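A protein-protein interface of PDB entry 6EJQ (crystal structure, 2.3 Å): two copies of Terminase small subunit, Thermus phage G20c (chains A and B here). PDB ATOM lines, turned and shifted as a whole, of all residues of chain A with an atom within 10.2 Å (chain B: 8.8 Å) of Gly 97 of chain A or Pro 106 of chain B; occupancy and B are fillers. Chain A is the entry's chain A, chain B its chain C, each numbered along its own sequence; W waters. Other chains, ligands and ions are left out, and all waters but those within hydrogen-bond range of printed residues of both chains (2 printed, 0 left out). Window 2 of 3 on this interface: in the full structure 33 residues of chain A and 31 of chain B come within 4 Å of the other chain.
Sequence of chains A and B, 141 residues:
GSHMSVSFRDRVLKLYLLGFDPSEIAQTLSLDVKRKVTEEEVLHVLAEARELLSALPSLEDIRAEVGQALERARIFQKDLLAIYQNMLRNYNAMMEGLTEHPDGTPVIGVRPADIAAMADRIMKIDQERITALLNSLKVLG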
ATOM      1  N   ARG A  89      -8.127  16.771  15.584  1.00  0.00           N
ATOM      2  CA  ARG A  89      -9.152  17.553  16.287  1.00  0.00           C
ATOM      3  C   ARG A  89      -9.560  18.759  15.434  1.00  0.00           C
ATOM      4  O   ARG A  89     -10.749  19.054  15.289  1.00  0.00           O
ATOM      5  CB  ARG A  89      -8.669  18.012  17.677  1.00  0.00           C
ATOM      6  CG  ARG A  89      -9.756  18.695  18.504  1.00  0.00           C
ATOM      7  CD  ARG A  89      -9.378  18.941  19.965  1.00  0.00           C
ATOM      8  NE  ARG A  89      -8.646  20.201  20.072  1.00  0.00           N
ATOM      9  CZ  ARG A  89      -8.988  21.278  20.776  1.00  0.00           C
ATOM     10  NH1 ARG A  89     -10.066  21.325  21.536  1.00  0.00           N
ATOM     11  NH2 ARG A  89      -8.199  22.335  20.728  1.00  0.00           N
ATOM     12  N   ASN A  90      -8.573  19.436  14.858  1.00  0.00           N
ATOM     13  CA  ASN A  90      -8.854  20.573  13.991  1.00  0.00           C
ATOM     14  C   ASN A  90      -9.605  20.153  12.734  1.00  0.00           C
ATOM     15  O   ASN A  90     -10.577  20.812  12.357  1.00  0.00           O
ATOM     16  CB  ASN A  90      -7.571  21.345  13.628  1.00  0.00           C
ATOM     17  CG  ASN A  90      -7.162  22.331  14.706  1.00  0.00           C
ATOM     18  OD1 ASN A  90      -5.990  22.440  15.055  1.00  0.00           O
ATOM     19  ND2 ASN A  90      -8.130  23.044  15.254  1.00  0.00           N
ATOM     20  N   TYR A  91      -9.178  19.052  12.119  1.00  0.00           N
ATOM     21  CA  TYR A  91      -9.790  18.569  10.889  1.00  0.00           C
ATOM     22  C   TYR A  91     -11.253  18.197  11.089  1.00  0.00           C
ATOM     23  O   TYR A  91     -12.094  18.540  10.264  1.00  0.00           O
ATOM     24  CB  TYR A  91      -9.022  17.363  10.324  1.00  0.00           C
ATOM     25  CG  TYR A  91      -9.639  16.821   9.055  1.00  0.00           C
ATOM     26  CD1 TYR A  91      -9.485  17.499   7.857  1.00  0.00           C
ATOM     27  CD2 TYR A  91     -10.401  15.649   9.058  1.00  0.00           C
ATOM     28  CE1 TYR A  91     -10.061  17.030   6.689  1.00  0.00           C
ATOM     29  CE2 TYR A  91     -10.989  15.172   7.891  1.00  0.00           C
ATOM     30  CZ  TYR A  91     -10.806  15.869   6.710  1.00  0.00           C
ATOM     31  OH  TYR A  91     -11.364  15.435   5.537  1.00  0.00           O
ATOM     32  N   ASN A  92     -11.549  17.483  12.172  1.00  0.00           N
ATOM     33  CA  ASN A  92     -12.933  17.079  12.469  1.00  0.00           C
ATOM     34  C   ASN A  92     -13.824  18.265  12.844  1.00  0.00           C
ATOM     35  O   ASN A  92     -14.983  18.310  12.447  1.00  0.00           O
ATOM     36  CB  ASN A  92     -12.973  15.997  13.553  1.00  0.00           C
ATOM     37  CG  ASN A  92     -12.401  14.683  13.071  1.00  0.00           C
ATOM     38  OD1 ASN A  92     -12.779  14.190  12.012  1.00  0.00           O
ATOM     39  ND2 ASN A  92     -11.484  14.112  13.832  1.00  0.00           N
ATOM     40  N   ALA A  93     -13.293  19.231  13.585  1.00  0.00           N
ATOM     41  CA  ALA A  93     -14.050  20.457  13.861  1.00  0.00           C
ATOM     42  C   ALA A  93     -14.370  21.209  12.565  1.00  0.00           C
ATOM     43  O   ALA A  93     -15.474  21.721  12.401  1.00  0.00           O
ATOM     44  CB  ALA A  93     -13.298  21.353  14.824  1.00  0.00           C
ATOM     45  N   MET A  94     -13.397  21.259  11.657  1.00  0.00           N
ATOM     46  CA  MET A  94     -13.569  21.839  10.313  1.00  0.00           C
ATOM     47  C   MET A  94     -14.686  21.133   9.530  1.00  0.00           C
ATOM     48  O   MET A  94     -15.538  21.773   8.922  1.00  0.00           O
ATOM     49  CB  MET A  94     -12.257  21.734   9.528  1.00  0.00           C
ATOM     50  CG  MET A  94     -11.806  22.996   8.830  1.00  0.00           C
ATOM     51  SD  MET A  94     -10.153  22.705   8.172  1.00  0.00           S
ATOM     52  CE  MET A  94     -10.509  21.704   6.720  1.00  0.00           C
ATOM     53  N   MET A  95     -14.667  19.805   9.572  1.00  0.00           N
ATOM     54  CA  MET A  95     -15.657  18.947   8.913  1.00  0.00           C
ATOM     55  C   MET A  95     -17.094  19.255   9.377  1.00  0.00           C
ATOM     56  O   MET A  95     -18.009  19.324   8.556  1.00  0.00           O
ATOM     57  CB  MET A  95     -15.292  17.471   9.175  1.00  0.00           C
ATOM     58  CG  MET A  95     -16.005  16.423   8.339  1.00  0.00           C
ATOM     59  SD  MET A  95     -15.515  14.732   8.788  1.00  0.00           S
ATOM     60  CE  MET A  95     -16.420  14.460  10.315  1.00  0.00           C
ATOM     61  N   GLU A  96     -17.290  19.468  10.679  1.00  0.00           N
ATOM     62  CA  GLU A  96     -18.634  19.767  11.205  1.00  0.00           C
ATOM     63  C   GLU A  96     -18.963  21.270  11.303  1.00  0.00           C
ATOM     64  O   GLU A  96     -19.935  21.648  11.952  1.00  0.00           O
ATOM     65  CB  GLU A  96     -18.906  19.002  12.516  1.00  0.00           C
ATOM     66  CG  GLU A  96     -18.193  19.488  13.766  1.00  0.00           C
ATOM     67  CD  GLU A  96     -18.375  18.531  14.942  1.00  0.00           C
ATOM     68  OE1 GLU A  96     -17.859  17.395  14.862  1.00  0.00           O
ATOM     69  OE2 GLU A  96     -19.034  18.903  15.944  1.00  0.00           O
ATOM     70  N   GLY A  97     -18.170  22.109  10.633  1.00  0.00           N
ATOM     71  CA  GLY A  97     -18.505  23.510  10.392  1.00  0.00           C
ATOM     72  C   GLY A  97     -18.118  24.512  11.463  1.00  0.00           C
ATOM     73  O   GLY A  97     -18.557  25.660  11.407  1.00  0.00           O
ATOM     74  N   LEU A  98     -17.274  24.106  12.411  1.00  0.00           N
ATOM     75  CA  LEU A  98     -16.984  24.907  13.602  1.00  0.00           C
ATOM     76  C   LEU A  98     -15.805  25.848  13.407  1.00  0.00           C
ATOM     77  O   LEU A  98     -14.803  25.481  12.805  1.00  0.00           O
ATOM     78  CB  LEU A  98     -16.689  23.991  14.792  1.00  0.00           C
ATOM     79  CG  LEU A  98     -17.800  23.016  15.201  1.00  0.00           C
ATOM     80  CD1 LEU A  98     -17.279  21.989  16.198  1.00  0.00           C
ATOM     81  CD2 LEU A  98     -19.001  23.763  15.775  1.00  0.00           C
ATOM     82  N   THR A  99     -15.940  27.067  13.917  1.00  0.00           N
ATOM     83  CA  THR A  99     -14.834  28.021  13.996  1.00  0.00           C
ATOM     84  C   THR A  99     -14.186  27.992  15.371  1.00  0.00           C
ATOM     85  O   THR A  99     -13.115  28.569  15.556  1.00  0.00           O
ATOM     86  CB  THR A  99     -15.304  29.470  13.729  1.00  0.00           C
ATOM     87  OG1 THR A  99     -16.384  29.799  14.613  1.00  0.00           O
ATOM     88  CG2 THR A  99     -15.763  29.625  12.295  1.00  0.00           C
ATOM     89  N   GLU A 100     -14.836  27.329  16.329  1.00  0.00           N
ATOM     90  CA  GLU A 100     -14.385  27.328  17.710  1.00  0.00           C
ATOM     91  C   GLU A 100     -14.548  25.918  18.280  1.00  0.00           C
ATOM     92  O   GLU A 100     -15.539  25.244  17.990  1.00  0.00           O
ATOM     93  CB  GLU A 100     -15.205  28.348  18.507  1.00  0.00           C
ATOM     94  CG  GLU A 100     -14.442  29.050  19.611  1.00  0.00           C
ATOM     95  CD  GLU A 100     -15.245  30.169  20.258  1.00  0.00           C
ATOM     96  OE1 GLU A 100     -16.339  29.878  20.793  1.00  0.00           O
ATOM     97  OE2 GLU A 100     -14.772  31.330  20.253  1.00  0.00           O
ATOM     98  N   HIS A 101     -13.557  25.473  19.055  1.00  0.00           N
ATOM     99  CA  HIS A 101     -13.612  24.178  19.746  1.00  0.00           C
ATOM    100  C   HIS A 101     -14.463  24.290  21.017  1.00  0.00           C
ATOM    101  O   HIS A 101     -14.656  25.402  21.524  1.00  0.00           O
ATOM    102  CB  HIS A 101     -12.208  23.713  20.142  1.00  0.00           C
ATOM    103  CG  HIS A 101     -11.362  23.305  18.986  1.00  0.00           C
ATOM    104  ND1 HIS A 101     -11.679  22.235  18.179  1.00  0.00           N
ATOM    105  CD2 HIS A 101     -10.219  23.835  18.488  1.00  0.00           C
ATOM    106  CE1 HIS A 101     -10.763  22.121  17.231  1.00  0.00           C
ATOM    107  NE2 HIS A 101      -9.864  23.074  17.402  1.00  0.00           N
ATOM    108  N   VAL A 107     -10.543  27.091  15.859  1.00  0.00           N
ATOM    109  CA  VAL A 107     -10.283  25.996  14.949  1.00  0.00           C
ATOM    110  C   VAL A 107      -9.278  26.517  13.921  1.00  0.00           C
ATOM    111  O   VAL A 107      -9.480  27.575  13.323  1.00  0.00           O
ATOM    112  CB  VAL A 107     -11.579  25.502  14.287  1.00  0.00           C
ATOM    113  CG1 VAL A 107     -11.287  24.422  13.260  1.00  0.00           C
ATOM    114  CG2 VAL A 107     -12.536  24.958  15.350  1.00  0.00           C
ATOM    115  N   ASN B  86     -14.286  11.134   3.649  1.00  0.00           N
ATOM    116  CA  ASN B  86     -14.728  12.532   3.787  1.00  0.00           C
ATOM    117  C   ASN B  86     -14.387  13.354   2.543  1.00  0.00           C
ATOM    118  O   ASN B  86     -15.192  14.174   2.101  1.00  0.00           O
ATOM    119  CB  ASN B  86     -14.084  13.224   5.006  1.00  0.00           C
ATOM    120  CG  ASN B  86     -14.256  12.447   6.298  1.00  0.00           C
ATOM    121  OD1 ASN B  86     -13.463  12.596   7.231  1.00  0.00           O
ATOM    122  ND2 ASN B  86     -15.289  11.616   6.362  1.00  0.00           N
ATOM    123  N   ARG B  89     -16.724  12.345  -0.267  1.00  0.00           N
ATOM    124  CA  ARG B  89     -18.036  12.923   0.053  1.00  0.00           C
ATOM    125  C   ARG B  89     -18.095  14.393  -0.358  1.00  0.00           C
ATOM    126  O   ARG B  89     -19.058  14.841  -0.968  1.00  0.00           O
ATOM    127  CB  ARG B  89     -18.357  12.772   1.544  1.00  0.00           C
ATOM    128  CG  ARG B  89     -19.795  13.104   1.925  1.00  0.00           C
ATOM    129  CD  ARG B  89     -20.096  12.743   3.375  1.00  0.00           C
ATOM    130  NE  ARG B  89     -19.563  13.760   4.293  1.00  0.00           N
ATOM    131  CZ  ARG B  89     -20.273  14.591   5.065  1.00  0.00           C
ATOM    132  NH1 ARG B  89     -21.609  14.559   5.097  1.00  0.00           N
ATOM    133  NH2 ARG B  89     -19.624  15.472   5.835  1.00  0.00           N
ATOM    134  N   ASN B  90     -17.043  15.130  -0.047  1.00  0.00           N
ATOM    135  CA  ASN B  90     -16.976  16.540  -0.396  1.00  0.00           C
ATOM    136  C   ASN B  90     -16.766  16.774  -1.895  1.00  0.00           C
ATOM    137  O   ASN B  90     -17.310  17.733  -2.444  1.00  0.00           O
ATOM    138  CB  ASN B  90     -15.893  17.244   0.422  1.00  0.00           C
ATOM    139  CG  ASN B  90     -16.351  17.566   1.827  1.00  0.00           C
ATOM    140  OD1 ASN B  90     -16.942  18.612   2.060  1.00  0.00           O
ATOM    141  ND2 ASN B  90     -16.087  16.672   2.763  1.00  0.00           N
ATOM    142  N   ALA B  93     -20.254  16.056  -3.555  1.00  0.00           N
ATOM    143  CA  ALA B  93     -21.160  17.175  -3.280  1.00  0.00           C
ATOM    144  C   ALA B  93     -20.776  18.416  -4.091  1.00  0.00           C
ATOM    145  O   ALA B  93     -21.636  19.063  -4.685  1.00  0.00           O
ATOM    146  CB  ALA B  93     -21.178  17.493  -1.791  1.00  0.00           C
ATOM    147  N   MET B  94     -19.483  18.733  -4.117  1.00  0.00           N
ATOM    148  CA  MET B  94     -18.938  19.843  -4.924  1.00  0.00           C
ATOM    149  C   MET B  94     -19.182  19.654  -6.423  1.00  0.00           C
ATOM    150  O   MET B  94     -19.329  20.631  -7.160  1.00  0.00           O
ATOM    151  CB  MET B  94     -17.432  19.963  -4.655  1.00  0.00           C
ATOM    152  CG  MET B  94     -16.694  21.115  -5.313  1.00  0.00           C
ATOM    153  SD  MET B  94     -14.923  20.950  -4.983  1.00  0.00           S
ATOM    154  CE  MET B  94     -14.320  22.560  -5.507  1.00  0.00           C
ATOM    155  N   LEU B  98     -23.315  21.718  -4.718  1.00  0.00           N
ATOM    156  CA  LEU B  98     -23.690  21.998  -3.323  1.00  0.00           C
ATOM    157  C   LEU B  98     -22.606  22.758  -2.555  1.00  0.00           C
ATOM    158  O   LEU B  98     -21.413  22.600  -2.831  1.00  0.00           O
ATOM    159  CB  LEU B  98     -24.009  20.691  -2.584  1.00  0.00           C
ATOM    160  CG  LEU B  98     -25.085  19.793  -3.200  1.00  0.00           C
ATOM    161  CD1 LEU B  98     -25.085  18.420  -2.553  1.00  0.00           C
ATOM    162  CD2 LEU B  98     -26.449  20.452  -3.074  1.00  0.00           C
ATOM    163  N   THR B  99     -23.040  23.601  -1.615  1.00  0.00           N
ATOM    164  CA  THR B  99     -22.151  24.254  -0.634  1.00  0.00           C
ATOM    165  C   THR B  99     -22.448  23.777   0.799  1.00  0.00           C
ATOM    166  O   THR B  99     -21.883  24.307   1.763  1.00  0.00           O
ATOM    167  CB  THR B  99     -22.267  25.796  -0.693  1.00  0.00           C
ATOM    168  OG1 THR B  99     -23.615  26.195  -0.416  1.00  0.00           O
ATOM    169  CG2 THR B  99     -21.848  26.322  -2.060  1.00  0.00           C
ATOM    170  N   GLU B 100     -23.300  22.758   0.925  1.00  0.00           N
ATOM    171  CA  GLU B 100     -23.821  22.319   2.213  1.00  0.00           C
ATOM    172  C   GLU B 100     -24.363  20.896   2.074  1.00  0.00           C
ATOM    173  O   GLU B 100     -25.096  20.601   1.135  1.00  0.00           O
ATOM    174  CB  GLU B 100     -24.927  23.280   2.662  1.00  0.00           C
ATOM    175  CG  GLU B 100     -25.518  23.013   4.039  1.00  0.00           C
ATOM    176  CD  GLU B 100     -26.608  24.010   4.417  1.00  0.00           C
ATOM    177  OE1 GLU B 100     -27.633  23.570   4.988  1.00  0.00           O
ATOM    178  OE2 GLU B 100     -26.444  25.226   4.144  1.00  0.00           O
ATOM    179  N   HIS B 101     -23.984  20.020   3.003  1.00  0.00           N
ATOM    180  CA  HIS B 101     -24.401  18.612   2.987  1.00  0.00           C
ATOM    181  C   HIS B 101     -25.844  18.479   3.488  1.00  0.00           C
ATOM    182  O   HIS B 101     -26.397  19.444   4.034  1.00  0.00           O
ATOM    183  CB  HIS B 101     -23.461  17.760   3.866  1.00  0.00           C
ATOM    184  CG  HIS B 101     -22.071  17.622   3.322  1.00  0.00           C
ATOM    185  ND1 HIS B 101     -20.988  18.270   3.877  1.00  0.00           N
ATOM    186  CD2 HIS B 101     -21.588  16.910   2.277  1.00  0.00           C
ATOM    187  CE1 HIS B 101     -19.900  17.968   3.195  1.00  0.00           C
ATOM    188  NE2 HIS B 101     -20.236  17.144   2.219  1.00  0.00           N
ATOM    189  N   PRO B 102     -26.462  17.290   3.308  1.00  0.00           N
ATOM    190  CA  PRO B 102     -27.785  17.033   3.890  1.00  0.00           C
ATOM    191  C   PRO B 102     -27.909  17.432   5.373  1.00  0.00           C
ATOM    192  O   PRO B 102     -28.845  18.148   5.743  1.00  0.00           O
ATOM    193  CB  PRO B 102     -27.946  15.518   3.716  1.00  0.00           C
ATOM    194  CG  PRO B 102     -27.195  15.217   2.466  1.00  0.00           C
ATOM    195  CD  PRO B 102     -26.036  16.178   2.431  1.00  0.00           C
ATOM    196  N   ASP B 103     -26.938  17.016   6.188  1.00  0.00           N
ATOM    197  CA  ASP B 103     -26.954  17.265   7.640  1.00  0.00           C
ATOM    198  C   ASP B 103     -26.506  18.675   8.088  1.00  0.00           C
ATOM    199  O   ASP B 103     -26.253  18.883   9.274  1.00  0.00           O
ATOM    200  CB  ASP B 103     -26.143  16.175   8.380  1.00  0.00           C
ATOM    201  CG  ASP B 103     -24.625  16.281   8.164  1.00  0.00           C
ATOM    202  OD1 ASP B 103     -24.164  16.965   7.223  1.00  0.00           O
ATOM    203  OD2 ASP B 103     -23.887  15.649   8.946  1.00  0.00           O
ATOM    204  N   GLY B 104     -26.396  19.629   7.161  1.00  0.00           N
ATOM    205  CA  GLY B 104     -26.067  21.014   7.508  1.00  0.00           C
ATOM    206  C   GLY B 104     -24.586  21.364   7.485  1.00  0.00           C
ATOM    207  O   GLY B 104     -24.238  22.547   7.484  1.00  0.00           O
ATOM    208  N   THR B 105     -23.713  20.351   7.440  1.00  0.00           N
ATOM    209  CA  THR B 105     -22.266  20.569   7.484  1.00  0.00           C
ATOM    210  C   THR B 105     -21.778  21.119   6.133  1.00  0.00           C
ATOM    211  O   THR B 105     -22.316  20.752   5.085  1.00  0.00           O
ATOM    212  CB  THR B 105     -21.499  19.273   7.833  1.00  0.00           C
ATOM    213  OG1 THR B 105     -21.703  18.287   6.816  1.00  0.00           O
ATOM    214  CG2 THR B 105     -21.947  18.708   9.184  1.00  0.00           C
ATOM    215  N   PRO B 106     -20.757  21.993   6.153  1.00  0.00           N
ATOM    216  CA  PRO B 106     -20.319  22.630   4.915  1.00  0.00           C
ATOM    217  C   PRO B 106     -19.584  21.679   3.962  1.00  0.00           C
ATOM    218  O   PRO B 106     -18.901  20.748   4.401  1.00  0.00           O
ATOM    219  CB  PRO B 106     -19.372  23.724   5.408  1.00  0.00           C
ATOM    220  CG  PRO B 106     -18.778  23.152   6.643  1.00  0.00           C
ATOM    221  CD  PRO B 106     -19.854  22.309   7.275  1.00  0.00           C
ATOM    222  N   VAL B 107     -19.754  21.928   2.666  1.00  0.00           N
ATOM    223  CA  VAL B 107     -19.007  21.251   1.620  1.00  0.00           C
ATOM    224  C   VAL B 107     -17.679  21.991   1.488  1.00  0.00           C
ATOM    225  O   VAL B 107     -17.666  23.168   1.149  1.00  0.00           O
ATOM    226  CB  VAL B 107     -19.780  21.260   0.287  1.00  0.00           C
ATOM    227  CG1 VAL B 107     -18.893  20.822  -0.874  1.00  0.00           C
ATOM    228  CG2 VAL B 107     -21.008  20.361   0.394  1.00  0.00           C
ATOM    229  N   ILE B 108     -16.579  21.299   1.780  1.00  0.00           N
ATOM    230  CA  ILE B 108     -15.226  21.863   1.710  1.00  0.00           C
ATOM    231  C   ILE B 108     -14.553  21.414   0.407  1.00  0.00           C
ATOM    232  O   ILE B 108     -14.679  20.265   0.005  1.00  0.00           O
ATOM    233  CB  ILE B 108     -14.395  21.445   2.945  1.00  0.00           C
ATOM    234  CG1 ILE B 108     -14.976  22.111   4.205  1.00  0.00           C
ATOM    235  CG2 ILE B 108     -12.918  21.819   2.784  1.00  0.00           C
ATOM    236  CD1 ILE B 108     -14.623  21.419   5.502  1.00  0.00           C
ATOM    237  N   GLY B 109     -13.838  22.333  -0.238  1.00  0.00           N
ATOM    238  CA  GLY B 109     -13.260  22.083  -1.552  1.00  0.00           C
ATOM    239  C   GLY B 109     -12.160  21.041  -1.512  1.00  0.00           C
ATOM    240  O   GLY B 109     -11.234  21.151  -0.706  1.00  0.00           O
HETATM  241  O   HOH W   1     -12.351  11.743  10.265  1.00  0.00           O
HETATM  242  O   HOH W   2     -17.743  18.804   5.925  1.00  0.00           O
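9 positions are printed for both chains. Of the 6 pairs that touch across the chains among the printed residues, none has its exchanged pair printed and touching as well.
The side-chain amide oxygen (OD1) of Asn 86 of chain B sits close to the side-chain sulfur (SD) of Met 95 of chain A (3.3 Å).
Hydrophobic or aromatic side chains of chain B within 4 Å of the printed part of chain A: Pro 106 and Ile 108. Of the 14 printed residues of chain A, 4 touch a printed residue of chain B. Hydrophobic or aromatic side chains of chain A within 4 Å of the printed part of chain B: Tyr 91 and Met 95. Among the printed residues, 6 pairs touch across the chains. Among the printed residues, no Asp or Glu carboxylate lies within 4 Å of a Lys or Arg side-chain nitrogen of the other chain.
Among the printed residues, pairs that only touch across the chains: Tyr 91 of chain A with Asn 86 of chain B (3.5 Å), Met 94 of chain A with Ile 108 of chain B (3.6 Å), Met 95 of chain A with Thr 105 of chain B (3.6 Å), Met 95 of chain A with Pro 106 of chain B (3.7 Å) and Gly 97 of chain A with Pro 106 of chain B (3.6 Å).
Pro 106 of chain B touches just these residues of chain A: Met 95 (3.7 Å) and Gly 97 (3.6 Å). Printed residues of chain A within 4 Å of Thr 105 of chain B: Met 95. No residue of chain A comes within 4 Å of Val 107 of chain B. Printed residues of chain B within 4 Å of Met 95 of chain A: Asn 86, Thr 105 and Pro 106. Printed residues of chain A within 4 Å of Asn 86 of chain B: Tyr 91 and Met 95. The nearest residue of chain A that does not touch Pro 106 of chain B is Met 94 of chain A (4.2 Å). The nearest printed residue of chain A that does not touch Ile 108 of chain B is Met 95 of chain A (4.3 Å).
Water W2 bridges the backbone carbonyl oxygen (O) of Met 95 of chain A (2.7 Å) and the backbone carbonyl oxygen (O) of Pro 106 of chain B (2.7 Å). Water W1 bridges the side-chain amide oxygen of Asn 92 of chain A (3.0 Å) and the side-chain amide oxygen of Asn 86 of chain B (3.3 Å).
A ring nitrogen (ND1) of His 101 of chain B sits at hydrogen-bond distance from the side-chain hydroxyl (OG1) of Thr 105 of chain B. ND1 of His 101 of chain B lies close to O of Pro 106 of chain B (3.3 Å). The backbone carbonyl oxygen (O) of Asn 86 of chain B lies within hydrogen-bond range of the side-chain amide nitrogen (ND2) of Asn 90 of chain B, 2.7 Å away. OD1 of Asp 103 of chain B lies within hydrogen-bond range of OG1 of Thr 105 of chain B. The side-chain amide oxygen (OD1) of Asn 90 of chain B is in hydrogen-bond range of the backbone NH (N) of Ile 108 of chain B (2.7 Å).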
